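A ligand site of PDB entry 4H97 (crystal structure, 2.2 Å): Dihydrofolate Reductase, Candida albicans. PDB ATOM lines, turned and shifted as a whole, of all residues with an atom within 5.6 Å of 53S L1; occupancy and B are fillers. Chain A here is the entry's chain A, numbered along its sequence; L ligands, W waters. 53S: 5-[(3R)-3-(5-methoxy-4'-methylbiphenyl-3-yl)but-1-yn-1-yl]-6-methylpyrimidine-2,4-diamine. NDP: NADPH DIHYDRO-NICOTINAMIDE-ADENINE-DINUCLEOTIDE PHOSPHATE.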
ATOM      1  N   ILE A   7     -24.903   9.494 -12.013  1.00  0.00           N
ATOM      2  CA  ILE A   7     -25.671   9.516 -13.257  1.00  0.00           C
ATOM      3  C   ILE A   7     -25.456   8.185 -13.987  1.00  0.00           C
ATOM      4  O   ILE A   7     -24.320   7.777 -14.236  1.00  0.00           O
ATOM      5  CB  ILE A   7     -25.377  10.777 -14.133  1.00  0.00           C
ATOM      6  CG1 ILE A   7     -26.332  10.847 -15.328  1.00  0.00           C
ATOM      7  CG2 ILE A   7     -23.905  10.833 -14.562  1.00  0.00           C
ATOM      8  CD1 ILE A   7     -26.396  12.198 -16.019  1.00  0.00           C
ATOM      9  N   VAL A   8     -26.558   7.511 -14.282  1.00  0.00           N
ATOM     10  CA  VAL A   8     -26.508   6.196 -14.909  1.00  0.00           C
ATOM     11  C   VAL A   8     -27.765   5.873 -15.710  1.00  0.00           C
ATOM     12  O   VAL A   8     -28.840   6.428 -15.460  1.00  0.00           O
ATOM     13  CB  VAL A   8     -26.250   5.080 -13.832  1.00  0.00           C
ATOM     14  CG1 VAL A   8     -27.386   5.044 -12.795  1.00  0.00           C
ATOM     15  CG2 VAL A   8     -26.041   3.711 -14.465  1.00  0.00           C
ATOM     16  N   ALA A   9     -27.614   5.014 -16.704  1.00  0.00           N
ATOM     17  CA  ALA A   9     -28.719   4.509 -17.504  1.00  0.00           C
ATOM     18  C   ALA A   9     -28.706   2.993 -17.384  1.00  0.00           C
ATOM     19  O   ALA A   9     -27.702   2.354 -17.693  1.00  0.00           O
ATOM     20  CB  ALA A   9     -28.579   4.959 -18.947  1.00  0.00           C
ATOM     21  N   MET A  23     -21.773  -0.837 -23.468  1.00  0.00           N
ATOM     22  CA  MET A  23     -23.206  -0.682 -23.218  1.00  0.00           C
ATOM     23  C   MET A  23     -24.004  -1.419 -24.288  1.00  0.00           C
ATOM     24  O   MET A  23     -23.705  -1.307 -25.477  1.00  0.00           O
ATOM     25  CB  MET A  23     -23.580   0.802 -23.162  1.00  0.00           C
ATOM     26  CG  MET A  23     -22.947   1.541 -21.991  1.00  0.00           C
ATOM     27  SD  MET A  23     -23.061   3.346 -22.100  1.00  0.00           S
ATOM     28  CE  MET A  23     -24.831   3.609 -22.024  1.00  0.00           C
ATOM     29  N   GLU A  30     -30.483  10.003 -25.060  1.00  0.00           N
ATOM     30  CA  GLU A  30     -29.978   9.776 -23.714  1.00  0.00           C
ATOM     31  C   GLU A  30     -28.528  10.265 -23.611  1.00  0.00           C
ATOM     32  O   GLU A  30     -28.145  10.896 -22.618  1.00  0.00           O
ATOM     33  CB  GLU A  30     -30.076   8.287 -23.347  1.00  0.00           C
ATOM     34  CG  GLU A  30     -30.261   7.989 -21.865  1.00  0.00           C
ATOM     35  CD  GLU A  30     -29.088   8.387 -20.993  1.00  0.00           C
ATOM     36  OE1 GLU A  30     -27.919   8.220 -21.418  1.00  0.00           O
ATOM     37  OE2 GLU A  30     -29.333   8.872 -19.865  1.00  0.00           O
ATOM     38  N   ILE A  31     -27.753   9.976 -24.649  1.00  0.00           N
ATOM     39  CA  ILE A  31     -26.367  10.424 -24.761  1.00  0.00           C
ATOM     40  C   ILE A  31     -26.286  11.950 -24.665  1.00  0.00           C
ATOM     41  O   ILE A  31     -25.392  12.496 -24.000  1.00  0.00           O
ATOM     42  CB  ILE A  31     -25.740   9.913 -26.093  1.00  0.00           C
ATOM     43  CG1 ILE A  31     -25.462   8.405 -25.995  1.00  0.00           C
ATOM     44  CG2 ILE A  31     -24.457  10.669 -26.439  1.00  0.00           C
ATOM     45  CD1 ILE A  31     -25.080   7.734 -27.317  1.00  0.00           C
ATOM     46  N   TYR A  33     -28.659  13.928 -23.285  1.00  0.00           N
ATOM     47  CA  TYR A  33     -29.103  14.266 -21.938  1.00  0.00           C
ATOM     48  C   TYR A  33     -27.914  14.215 -20.984  1.00  0.00           C
ATOM     49  O   TYR A  33     -27.696  15.144 -20.191  1.00  0.00           O
ATOM     50  CB  TYR A  33     -30.199  13.289 -21.492  1.00  0.00           C
ATOM     51  CG  TYR A  33     -30.591  13.350 -20.026  1.00  0.00           C
ATOM     52  CD1 TYR A  33     -31.567  14.248 -19.582  1.00  0.00           C
ATOM     53  CD2 TYR A  33     -30.014  12.488 -19.094  1.00  0.00           C
ATOM     54  CE1 TYR A  33     -31.935  14.299 -18.250  1.00  0.00           C
ATOM     55  CE2 TYR A  33     -30.379  12.529 -17.753  1.00  0.00           C
ATOM     56  CZ  TYR A  33     -31.343  13.436 -17.334  1.00  0.00           C
ATOM     57  OH  TYR A  33     -31.713  13.484 -16.016  1.00  0.00           O
ATOM     58  N   PHE A  34     -27.147  13.134 -21.075  1.00  0.00           N
ATOM     59  CA  PHE A  34     -25.938  12.936 -20.268  1.00  0.00           C
ATOM     60  C   PHE A  34     -24.950  14.089 -20.420  1.00  0.00           C
ATOM     61  O   PHE A  34     -24.398  14.576 -19.430  1.00  0.00           O
ATOM     62  CB  PHE A  34     -25.270  11.605 -20.640  1.00  0.00           C
ATOM     63  CG  PHE A  34     -23.882  11.446 -20.083  1.00  0.00           C
ATOM     64  CD1 PHE A  34     -23.688  11.037 -18.771  1.00  0.00           C
ATOM     65  CD2 PHE A  34     -22.764  11.709 -20.874  1.00  0.00           C
ATOM     66  CE1 PHE A  34     -22.405  10.884 -18.249  1.00  0.00           C
ATOM     67  CE2 PHE A  34     -21.479  11.561 -20.368  1.00  0.00           C
ATOM     68  CZ  PHE A  34     -21.302  11.151 -19.053  1.00  0.00           C
ATOM     69  N   LYS A  35     -24.746  14.540 -21.660  1.00  0.00           N
ATOM     70  CA  LYS A  35     -23.808  15.619 -21.949  1.00  0.00           C
ATOM     71  C   LYS A  35     -24.265  16.958 -21.364  1.00  0.00           C
ATOM     72  O   LYS A  35     -23.486  17.639 -20.695  1.00  0.00           O
ATOM     73  CB  LYS A  35     -23.558  15.732 -23.459  1.00  0.00           C
ATOM     74  CG  LYS A  35     -22.508  16.768 -23.852  1.00  0.00           C
ATOM     75  CD  LYS A  35     -22.221  16.753 -25.341  1.00  0.00           C
ATOM     76  CE  LYS A  35     -23.474  17.014 -26.154  1.00  0.00           C
ATOM     77  NZ  LYS A  35     -24.471  15.925 -25.971  1.00  0.00           N
ATOM     78  N   MET A  52     -14.829   9.050 -12.802  1.00  0.00           N
ATOM     79  CA  MET A  52     -14.997   7.748 -13.433  1.00  0.00           C
ATOM     80  C   MET A  52     -13.879   6.792 -13.059  1.00  0.00           C
ATOM     81  O   MET A  52     -12.813   7.208 -12.606  1.00  0.00           O
ATOM     82  CB  MET A  52     -15.085   7.910 -14.958  1.00  0.00           C
ATOM     83  CG  MET A  52     -13.748   8.171 -15.666  1.00  0.00           C
ATOM     84  SD  MET A  52     -13.952   8.917 -17.286  1.00  0.00           S
ATOM     85  CE  MET A  52     -14.148  10.639 -16.828  1.00  0.00           C
ATOM     86  N   THR A  56     -13.388   2.721 -17.343  1.00  0.00           N
ATOM     87  CA  THR A  56     -14.364   3.530 -18.081  1.00  0.00           C
ATOM     88  C   THR A  56     -13.643   4.591 -18.925  1.00  0.00           C
ATOM     89  O   THR A  56     -14.016   4.821 -20.081  1.00  0.00           O
ATOM     90  CB  THR A  56     -15.390   4.204 -17.139  1.00  0.00           C
ATOM     91  OG1 THR A  56     -16.112   3.186 -16.430  1.00  0.00           O
ATOM     92  CG2 THR A  56     -16.369   5.050 -17.922  1.00  0.00           C
ATOM     93  N   SER A  59     -12.236   3.143 -22.075  1.00  0.00           N
ATOM     94  CA  SER A  59     -13.257   2.722 -23.025  1.00  0.00           C
ATOM     95  C   SER A  59     -13.729   3.876 -23.908  1.00  0.00           C
ATOM     96  O   SER A  59     -14.201   3.662 -25.037  1.00  0.00           O
ATOM     97  CB  SER A  59     -14.457   2.097 -22.303  1.00  0.00           C
ATOM     98  OG  SER A  59     -15.174   3.063 -21.557  1.00  0.00           O
ATOM     99  N   ILE A  60     -13.607   5.097 -23.391  1.00  0.00           N
ATOM    100  CA  ILE A  60     -14.003   6.311 -24.093  1.00  0.00           C
ATOM    101  C   ILE A  60     -13.078   6.575 -25.292  1.00  0.00           C
ATOM    102  O   ILE A  60     -11.856   6.549 -25.141  1.00  0.00           O
ATOM    103  CB  ILE A  60     -14.020   7.538 -23.144  1.00  0.00           C
ATOM    104  CG1 ILE A  60     -14.994   7.303 -21.988  1.00  0.00           C
ATOM    105  CG2 ILE A  60     -14.366   8.830 -23.887  1.00  0.00           C
ATOM    106  CD1 ILE A  60     -14.932   8.346 -20.886  1.00  0.00           C
ATOM    107  N   PRO A  61     -13.674   6.799 -26.484  1.00  0.00           N
ATOM    108  CA  PRO A  61     -12.924   7.078 -27.717  1.00  0.00           C
ATOM    109  C   PRO A  61     -11.965   8.268 -27.586  1.00  0.00           C
ATOM    110  O   PRO A  61     -12.314   9.277 -26.975  1.00  0.00           O
ATOM    111  CB  PRO A  61     -14.036   7.396 -28.720  1.00  0.00           C
ATOM    112  CG  PRO A  61     -15.197   6.618 -28.242  1.00  0.00           C
ATOM    113  CD  PRO A  61     -15.126   6.666 -26.746  1.00  0.00           C
ATOM    114  N   PHE A  64     -13.075  11.890 -27.751  1.00  0.00           N
ATOM    115  CA  PHE A  64     -14.072  12.280 -26.758  1.00  0.00           C
ATOM    116  C   PHE A  64     -13.490  12.394 -25.346  1.00  0.00           C
ATOM    117  O   PHE A  64     -14.188  12.795 -24.411  1.00  0.00           O
ATOM    118  CB  PHE A  64     -15.272  11.312 -26.752  1.00  0.00           C
ATOM    119  CG  PHE A  64     -16.096  11.340 -28.010  1.00  0.00           C
ATOM    120  CD1 PHE A  64     -16.780  12.487 -28.386  1.00  0.00           C
ATOM    121  CD2 PHE A  64     -16.214  10.200 -28.802  1.00  0.00           C
ATOM    122  CE1 PHE A  64     -17.553  12.513 -29.549  1.00  0.00           C
ATOM    123  CE2 PHE A  64     -16.979  10.211 -29.962  1.00  0.00           C
ATOM    124  CZ  PHE A  64     -17.646  11.371 -30.338  1.00  0.00           C
ATOM    125  N   LEU A  67     -13.665  14.441 -21.421  1.00  0.00           N
ATOM    126  CA  LEU A  67     -14.993  14.987 -21.729  1.00  0.00           C
ATOM    127  C   LEU A  67     -14.921  16.513 -21.652  1.00  0.00           C
ATOM    128  O   LEU A  67     -14.589  17.060 -20.603  1.00  0.00           O
ATOM    129  CB  LEU A  67     -16.068  14.407 -20.809  1.00  0.00           C
ATOM    130  CG  LEU A  67     -16.332  12.897 -20.872  1.00  0.00           C
ATOM    131  CD1 LEU A  67     -17.341  12.480 -19.816  1.00  0.00           C
ATOM    132  CD2 LEU A  67     -16.806  12.453 -22.259  1.00  0.00           C
ATOM    133  N   ILE A 109     -20.797  11.194 -10.858  1.00  0.00           N
ATOM    134  CA  ILE A 109     -20.178   9.883 -10.963  1.00  0.00           C
ATOM    135  C   ILE A 109     -20.775   9.242 -12.212  1.00  0.00           C
ATOM    136  O   ILE A 109     -21.992   9.077 -12.300  1.00  0.00           O
ATOM    137  CB  ILE A 109     -20.419   9.033  -9.702  1.00  0.00           C
ATOM    138  CG1 ILE A 109     -19.697   9.674  -8.509  1.00  0.00           C
ATOM    139  CG2 ILE A 109     -19.966   7.597  -9.913  1.00  0.00           C
ATOM    140  CD1 ILE A 109     -20.119   9.141  -7.156  1.00  0.00           C
ATOM    141  N   ILE A 110     -19.922   8.915 -13.181  1.00  0.00           N
ATOM    142  CA  ILE A 110     -20.404   8.430 -14.484  1.00  0.00           C
ATOM    143  C   ILE A 110     -20.061   6.969 -14.796  1.00  0.00           C
ATOM    144  O   ILE A 110     -20.301   6.514 -15.910  1.00  0.00           O
ATOM    145  CB  ILE A 110     -19.925   9.359 -15.640  1.00  0.00           C
ATOM    146  CG1 ILE A 110     -18.405   9.324 -15.807  1.00  0.00           C
ATOM    147  CG2 ILE A 110     -20.422  10.791 -15.414  1.00  0.00           C
ATOM    148  CD1 ILE A 110     -17.882  10.088 -17.007  1.00  0.00           C
ATOM    149  N   GLY A 111     -19.506   6.244 -13.825  1.00  0.00           N
ATOM    150  CA  GLY A 111     -19.179   4.821 -14.018  1.00  0.00           C
ATOM    151  C   GLY A 111     -17.743   4.419 -13.774  1.00  0.00           C
ATOM    152  O   GLY A 111     -16.920   5.245 -13.402  1.00  0.00           O
ATOM    153  N   TYR A 116     -19.910   2.559  -9.439  1.00  0.00           N
ATOM    154  CA  TYR A 116     -21.300   2.748  -8.997  1.00  0.00           C
ATOM    155  C   TYR A 116     -21.600   1.963  -7.726  1.00  0.00           C
ATOM    156  O   TYR A 116     -22.019   2.533  -6.713  1.00  0.00           O
ATOM    157  CB  TYR A 116     -22.307   2.314 -10.072  1.00  0.00           C
ATOM    158  CG  TYR A 116     -22.368   3.127 -11.356  1.00  0.00           C
ATOM    159  CD1 TYR A 116     -22.585   4.503 -11.324  1.00  0.00           C
ATOM    160  CD2 TYR A 116     -22.295   2.495 -12.592  1.00  0.00           C
ATOM    161  CE1 TYR A 116     -22.673   5.231 -12.505  1.00  0.00           C
ATOM    162  CE2 TYR A 116     -22.383   3.210 -13.777  1.00  0.00           C
ATOM    163  CZ  TYR A 116     -22.579   4.579 -13.725  1.00  0.00           C
ATOM    164  OH  TYR A 116     -22.660   5.292 -14.904  1.00  0.00           O
ATOM    165  N   LEU A 129     -29.296  10.100 -10.558  1.00  0.00           N
ATOM    166  CA  LEU A 129     -29.949  10.396 -11.830  1.00  0.00           C
ATOM    167  C   LEU A 129     -29.927   9.121 -12.651  1.00  0.00           C
ATOM    168  O   LEU A 129     -28.955   8.827 -13.361  1.00  0.00           O
ATOM    169  CB  LEU A 129     -29.275  11.562 -12.557  1.00  0.00           C
ATOM    170  CG  LEU A 129     -29.483  12.976 -12.014  1.00  0.00           C
ATOM    171  CD1 LEU A 129     -28.673  13.241 -10.746  1.00  0.00           C
ATOM    172  CD2 LEU A 129     -29.108  13.989 -13.076  1.00  0.00           C
ATOM    173  N   THR A 131     -31.559   6.737 -15.547  1.00  0.00           N
ATOM    174  CA  THR A 131     -32.378   6.665 -16.725  1.00  0.00           C
ATOM    175  C   THR A 131     -32.888   5.230 -16.771  1.00  0.00           C
ATOM    176  O   THR A 131     -32.135   4.304 -17.093  1.00  0.00           O
ATOM    177  CB  THR A 131     -31.618   7.029 -18.014  1.00  0.00           C
ATOM    178  OG1 THR A 131     -31.177   8.383 -17.938  1.00  0.00           O
ATOM    179  CG2 THR A 131     -32.533   6.873 -19.224  1.00  0.00           C
HETATM  180  C6  53S L   1     -23.531   7.522 -19.192  1.00  0.00           C
HETATM  181  C5  53S L   1     -24.525   7.719 -20.152  1.00  0.00           C
HETATM  182  C2  53S L   1     -18.114   3.946 -24.469  1.00  0.00           C
HETATM  183  C20 53S L   1     -21.154  10.003 -24.118  1.00  0.00           C
HETATM  184  C21 53S L   1     -21.585  11.173 -24.724  1.00  0.00           C
HETATM  185  C22 53S L   1     -20.717  11.886 -25.558  1.00  0.00           C
HETATM  186  C26 53S L   1     -21.199  13.175 -26.234  1.00  0.00           C
HETATM  187  C23 53S L   1     -19.421  11.425 -25.770  1.00  0.00           C
HETATM  188  C24 53S L   1     -18.988  10.259 -25.151  1.00  0.00           C
HETATM  189  C25 53S L   1     -19.844   9.538 -24.316  1.00  0.00           C
HETATM  190  C18 53S L   1     -19.434   8.349 -23.695  1.00  0.00           C
HETATM  191  C19 53S L   1     -19.737   8.106 -22.353  1.00  0.00           C
HETATM  192  C17 53S L   1     -18.726   7.393 -24.428  1.00  0.00           C
HETATM  193  C16 53S L   1     -18.313   6.196 -23.827  1.00  0.00           C
HETATM  194  O17 53S L   1     -17.607   5.291 -24.556  1.00  0.00           O
HETATM  195  C15 53S L   1     -18.616   5.980 -22.476  1.00  0.00           C
HETATM  196  C14 53S L   1     -19.334   6.920 -21.738  1.00  0.00           C
HETATM  197  C12 53S L   1     -19.643   6.612 -20.263  1.00  0.00           C
HETATM  198  C13 53S L   1     -18.683   7.410 -19.371  1.00  0.00           C
HETATM  199  C11 53S L   1     -21.031   6.936 -19.896  1.00  0.00           C
HETATM  200  C10 53S L   1     -22.187   7.206 -19.584  1.00  0.00           C
HETATM  201  C8  53S L   1     -24.220   7.604 -21.650  1.00  0.00           C
HETATM  202  N4  53S L   1     -25.768   8.009 -19.757  1.00  0.00           N
HETATM  203  C3  53S L   1     -26.077   8.126 -18.449  1.00  0.00           C
HETATM  204  N7  53S L   1     -27.330   8.412 -18.088  1.00  0.00           N
HETATM  205  N2  53S L   1     -25.132   7.943 -17.506  1.00  0.00           N
HETATM  206  C1  53S L   1     -23.869   7.644 -17.852  1.00  0.00           C
HETATM  207  N9  53S L   1     -22.969   7.471 -16.890  1.00  0.00           N
HETATM  208  PA  NDP L   2     -14.876   0.861 -13.873  1.00  0.00           P
HETATM  209  O1A NDP L   2     -15.771   0.790 -12.700  1.00  0.00           O
HETATM  210  O2A NDP L   2     -14.988   2.177 -14.542  1.00  0.00           O
HETATM  211  O5B NDP L   2     -13.354   0.588 -13.482  1.00  0.00           O
HETATM  212  C5B NDP L   2     -13.003  -0.083 -12.291  1.00  0.00           C
HETATM  213  C4B NDP L   2     -11.649   0.483 -11.911  1.00  0.00           C
HETATM  214  O4B NDP L   2     -11.812   1.659 -11.139  1.00  0.00           O
HETATM  215  C3B NDP L   2     -10.834  -0.487 -11.074  1.00  0.00           C
HETATM  216  O3B NDP L   2     -10.071  -1.341 -11.875  1.00  0.00           O
HETATM  217  C2B NDP L   2     -10.002   0.455 -10.252  1.00  0.00           C
HETATM  218  O2B NDP L   2      -8.848   0.850 -10.945  1.00  0.00           O
HETATM  219  C1B NDP L   2     -10.886   1.679 -10.063  1.00  0.00           C
HETATM  220  N9A NDP L   2     -11.616   1.650  -8.779  1.00  0.00           N
HETATM  221  C8A NDP L   2     -12.686   0.861  -8.459  1.00  0.00           C
HETATM  222  N7A NDP L   2     -13.079   1.137  -7.202  1.00  0.00           N
HETATM  223  C5A NDP L   2     -12.266   2.099  -6.697  1.00  0.00           C
HETATM  224  C6A NDP L   2     -12.224   2.740  -5.474  1.00  0.00           C
HETATM  225  N6A NDP L   2     -13.114   2.421  -4.525  1.00  0.00           N
HETATM  226  N1A NDP L   2     -11.270   3.710  -5.235  1.00  0.00           N
HETATM  227  C2A NDP L   2     -10.357   4.026  -6.224  1.00  0.00           C
HETATM  228  N3A NDP L   2     -10.399   3.385  -7.447  1.00  0.00           N
HETATM  229  C4A NDP L   2     -11.348   2.437  -7.684  1.00  0.00           C
HETATM  230  O3  NDP L   2     -15.168  -0.332 -14.904  1.00  0.00           O
HETATM  231  PN  NDP L   2     -16.089  -1.642 -14.801  1.00  0.00           P
HETATM  232  O1N NDP L   2     -15.444  -2.732 -15.575  1.00  0.00           O
HETATM  233  O2N NDP L   2     -16.450  -1.859 -13.375  1.00  0.00           O
HETATM  234  O5D NDP L   2     -17.412  -1.163 -15.572  1.00  0.00           O
HETATM  235  C5D NDP L   2     -17.465  -1.134 -16.985  1.00  0.00           C
HETATM  236  C4D NDP L   2     -18.893  -1.446 -17.409  1.00  0.00           C
HETATM  237  O4D NDP L   2     -19.754  -0.420 -16.952  1.00  0.00           O
HETATM  238  C3D NDP L   2     -19.062  -1.543 -18.907  1.00  0.00           C
HETATM  239  O3D NDP L   2     -19.629  -2.783 -19.259  1.00  0.00           O
HETATM  240  C2D NDP L   2     -20.009  -0.426 -19.285  1.00  0.00           C
HETATM  241  O2D NDP L   2     -20.950  -0.840 -20.243  1.00  0.00           O
HETATM  242  C1D NDP L   2     -20.680  -0.075 -17.963  1.00  0.00           C
HETATM  243  N1N NDP L   2     -21.066   1.352 -17.915  1.00  0.00           N
HETATM  244  C2N NDP L   2     -22.374   1.665 -18.145  1.00  0.00           C
HETATM  245  C3N NDP L   2     -22.805   2.983 -18.102  1.00  0.00           C
HETATM  246  C7N NDP L   2     -24.277   3.285 -18.193  1.00  0.00           C
HETATM  247  O7N NDP L   2     -24.766   4.525 -17.713  1.00  0.00           O
HETATM  248  N7N NDP L   2     -25.101   2.384 -18.724  1.00  0.00           N
HETATM  249  C4N NDP L   2     -21.884   3.990 -17.815  1.00  0.00           C
HETATM  250  C5N NDP L   2     -20.550   3.665 -17.572  1.00  0.00           C
HETATM  251  C6N NDP L   2     -20.149   2.327 -17.620  1.00  0.00           C
HETATM  252  P2B NDP L   2      -7.417   0.140 -10.713  1.00  0.00           P
HETATM  253  O1X NDP L   2      -6.418   0.797 -11.616  1.00  0.00           O
HETATM  254  O2X NDP L   2      -7.007   0.299  -9.268  1.00  0.00           O
HETATM  255  O3X NDP L   2      -7.542  -1.329 -11.058  1.00  0.00           O
HETATM  256  O   HOH W   1     -20.781  13.819 -22.866  1.00  0.00           O
HETATM  257  O   HOH W   2     -19.015  14.966 -24.544  1.00  0.00           O
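A nitrogen (N7) of 53S L1 sits at hydrogen-bond distance from the side-chain carboxylate (OE2) of Glu 30. A nitrogen (N9) of 53S L1 lies within hydrogen-bond range of the side-chain hydroxyl of Tyr 116, at 3.0 Å. N9 of 53S L1 sits at hydrogen-bond distance from O of Ile 7, at 3.0 Å. O of Ile 110 lies within hydrogen-bond range of N9 of 53S L1 (3.0 Å). The backbone NH (N) of Thr 56 is in hydrogen-bond range of an oxygen (O2A) of NDP L2 (3.3 Å). The side-chain hydroxyl (OG1) of Thr 56 lies within hydrogen-bond range of an oxygen (O2A) of NDP L2, 2.4 Å away. N of Ala 9 lies within hydrogen-bond range of O7N of NDP L2 (3.1 Å). O of Ala 9 sits at hydrogen-bond distance from N7N of NDP L2 (2.8 Å). An oxygen (O2D) of NDP L2 lies within hydrogen-bond range of the backbone NH (N) of Met 23, 3.3 Å away.
OE2 of Glu 30 is in hydrogen-bond range of OG1 of Thr 131. The side-chain hydroxyl (OH) of Tyr 116 lies within hydrogen-bond range of the backbone carbonyl oxygen (O) of Ile 7, 3.1 Å away. OH of Tyr 116 is in hydrogen-bond range of O of Ile 110. N of Gly 111 is in hydrogen-bond range of OH of Tyr 116 (3.5 Å). The backbone NH (N) of Ile 7 lies within hydrogen-bond range of the backbone carbonyl oxygen (O) of Ile 109 (3.0 Å). The backbone NH (N) of Thr 131 lies within hydrogen-bond range of the backbone carbonyl oxygen (O) of Val 8 (2.7 Å). O of Leu 129 sits at hydrogen-bond distance from N of Val 8 (2.9 Å). The side-chain hydroxyl (OG) of Ser 59 sits at hydrogen-bond distance from the backbone carbonyl oxygen (O) of Thr 56 (2.6 Å).
Merely in contact with 53S L1: Ile 31 (3.4 Å), Val 8 (3.4 Å), Phe 34 (3.5 Å), Pro 61 (3.6 Å), Thr 56 (3.6 Å), Ala 9 (3.7 Å), Ile 60 (3.8 Å), Ser 59 (3.8 Å), Lys 35 (3.8 Å), Thr 131 (3.9 Å) and Phe 64 (3.9 Å). Hydrophobic or aromatic side chains that line 53S L1: Ile 7, Ala 9, Ile 31, Phe 34, Ile 60, Pro 61, Phe 64 and Ile 110. 15 residues have an atom within 4 Å of 53S L1: Ile 7, Val 8, Ala 9, Glu 30, Ile 31, Phe 34, Lys 35, Thr 56, Ser 59, Ile 60, Pro 61, Phe 64, Ile 110, Tyr 116 and Thr 131.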
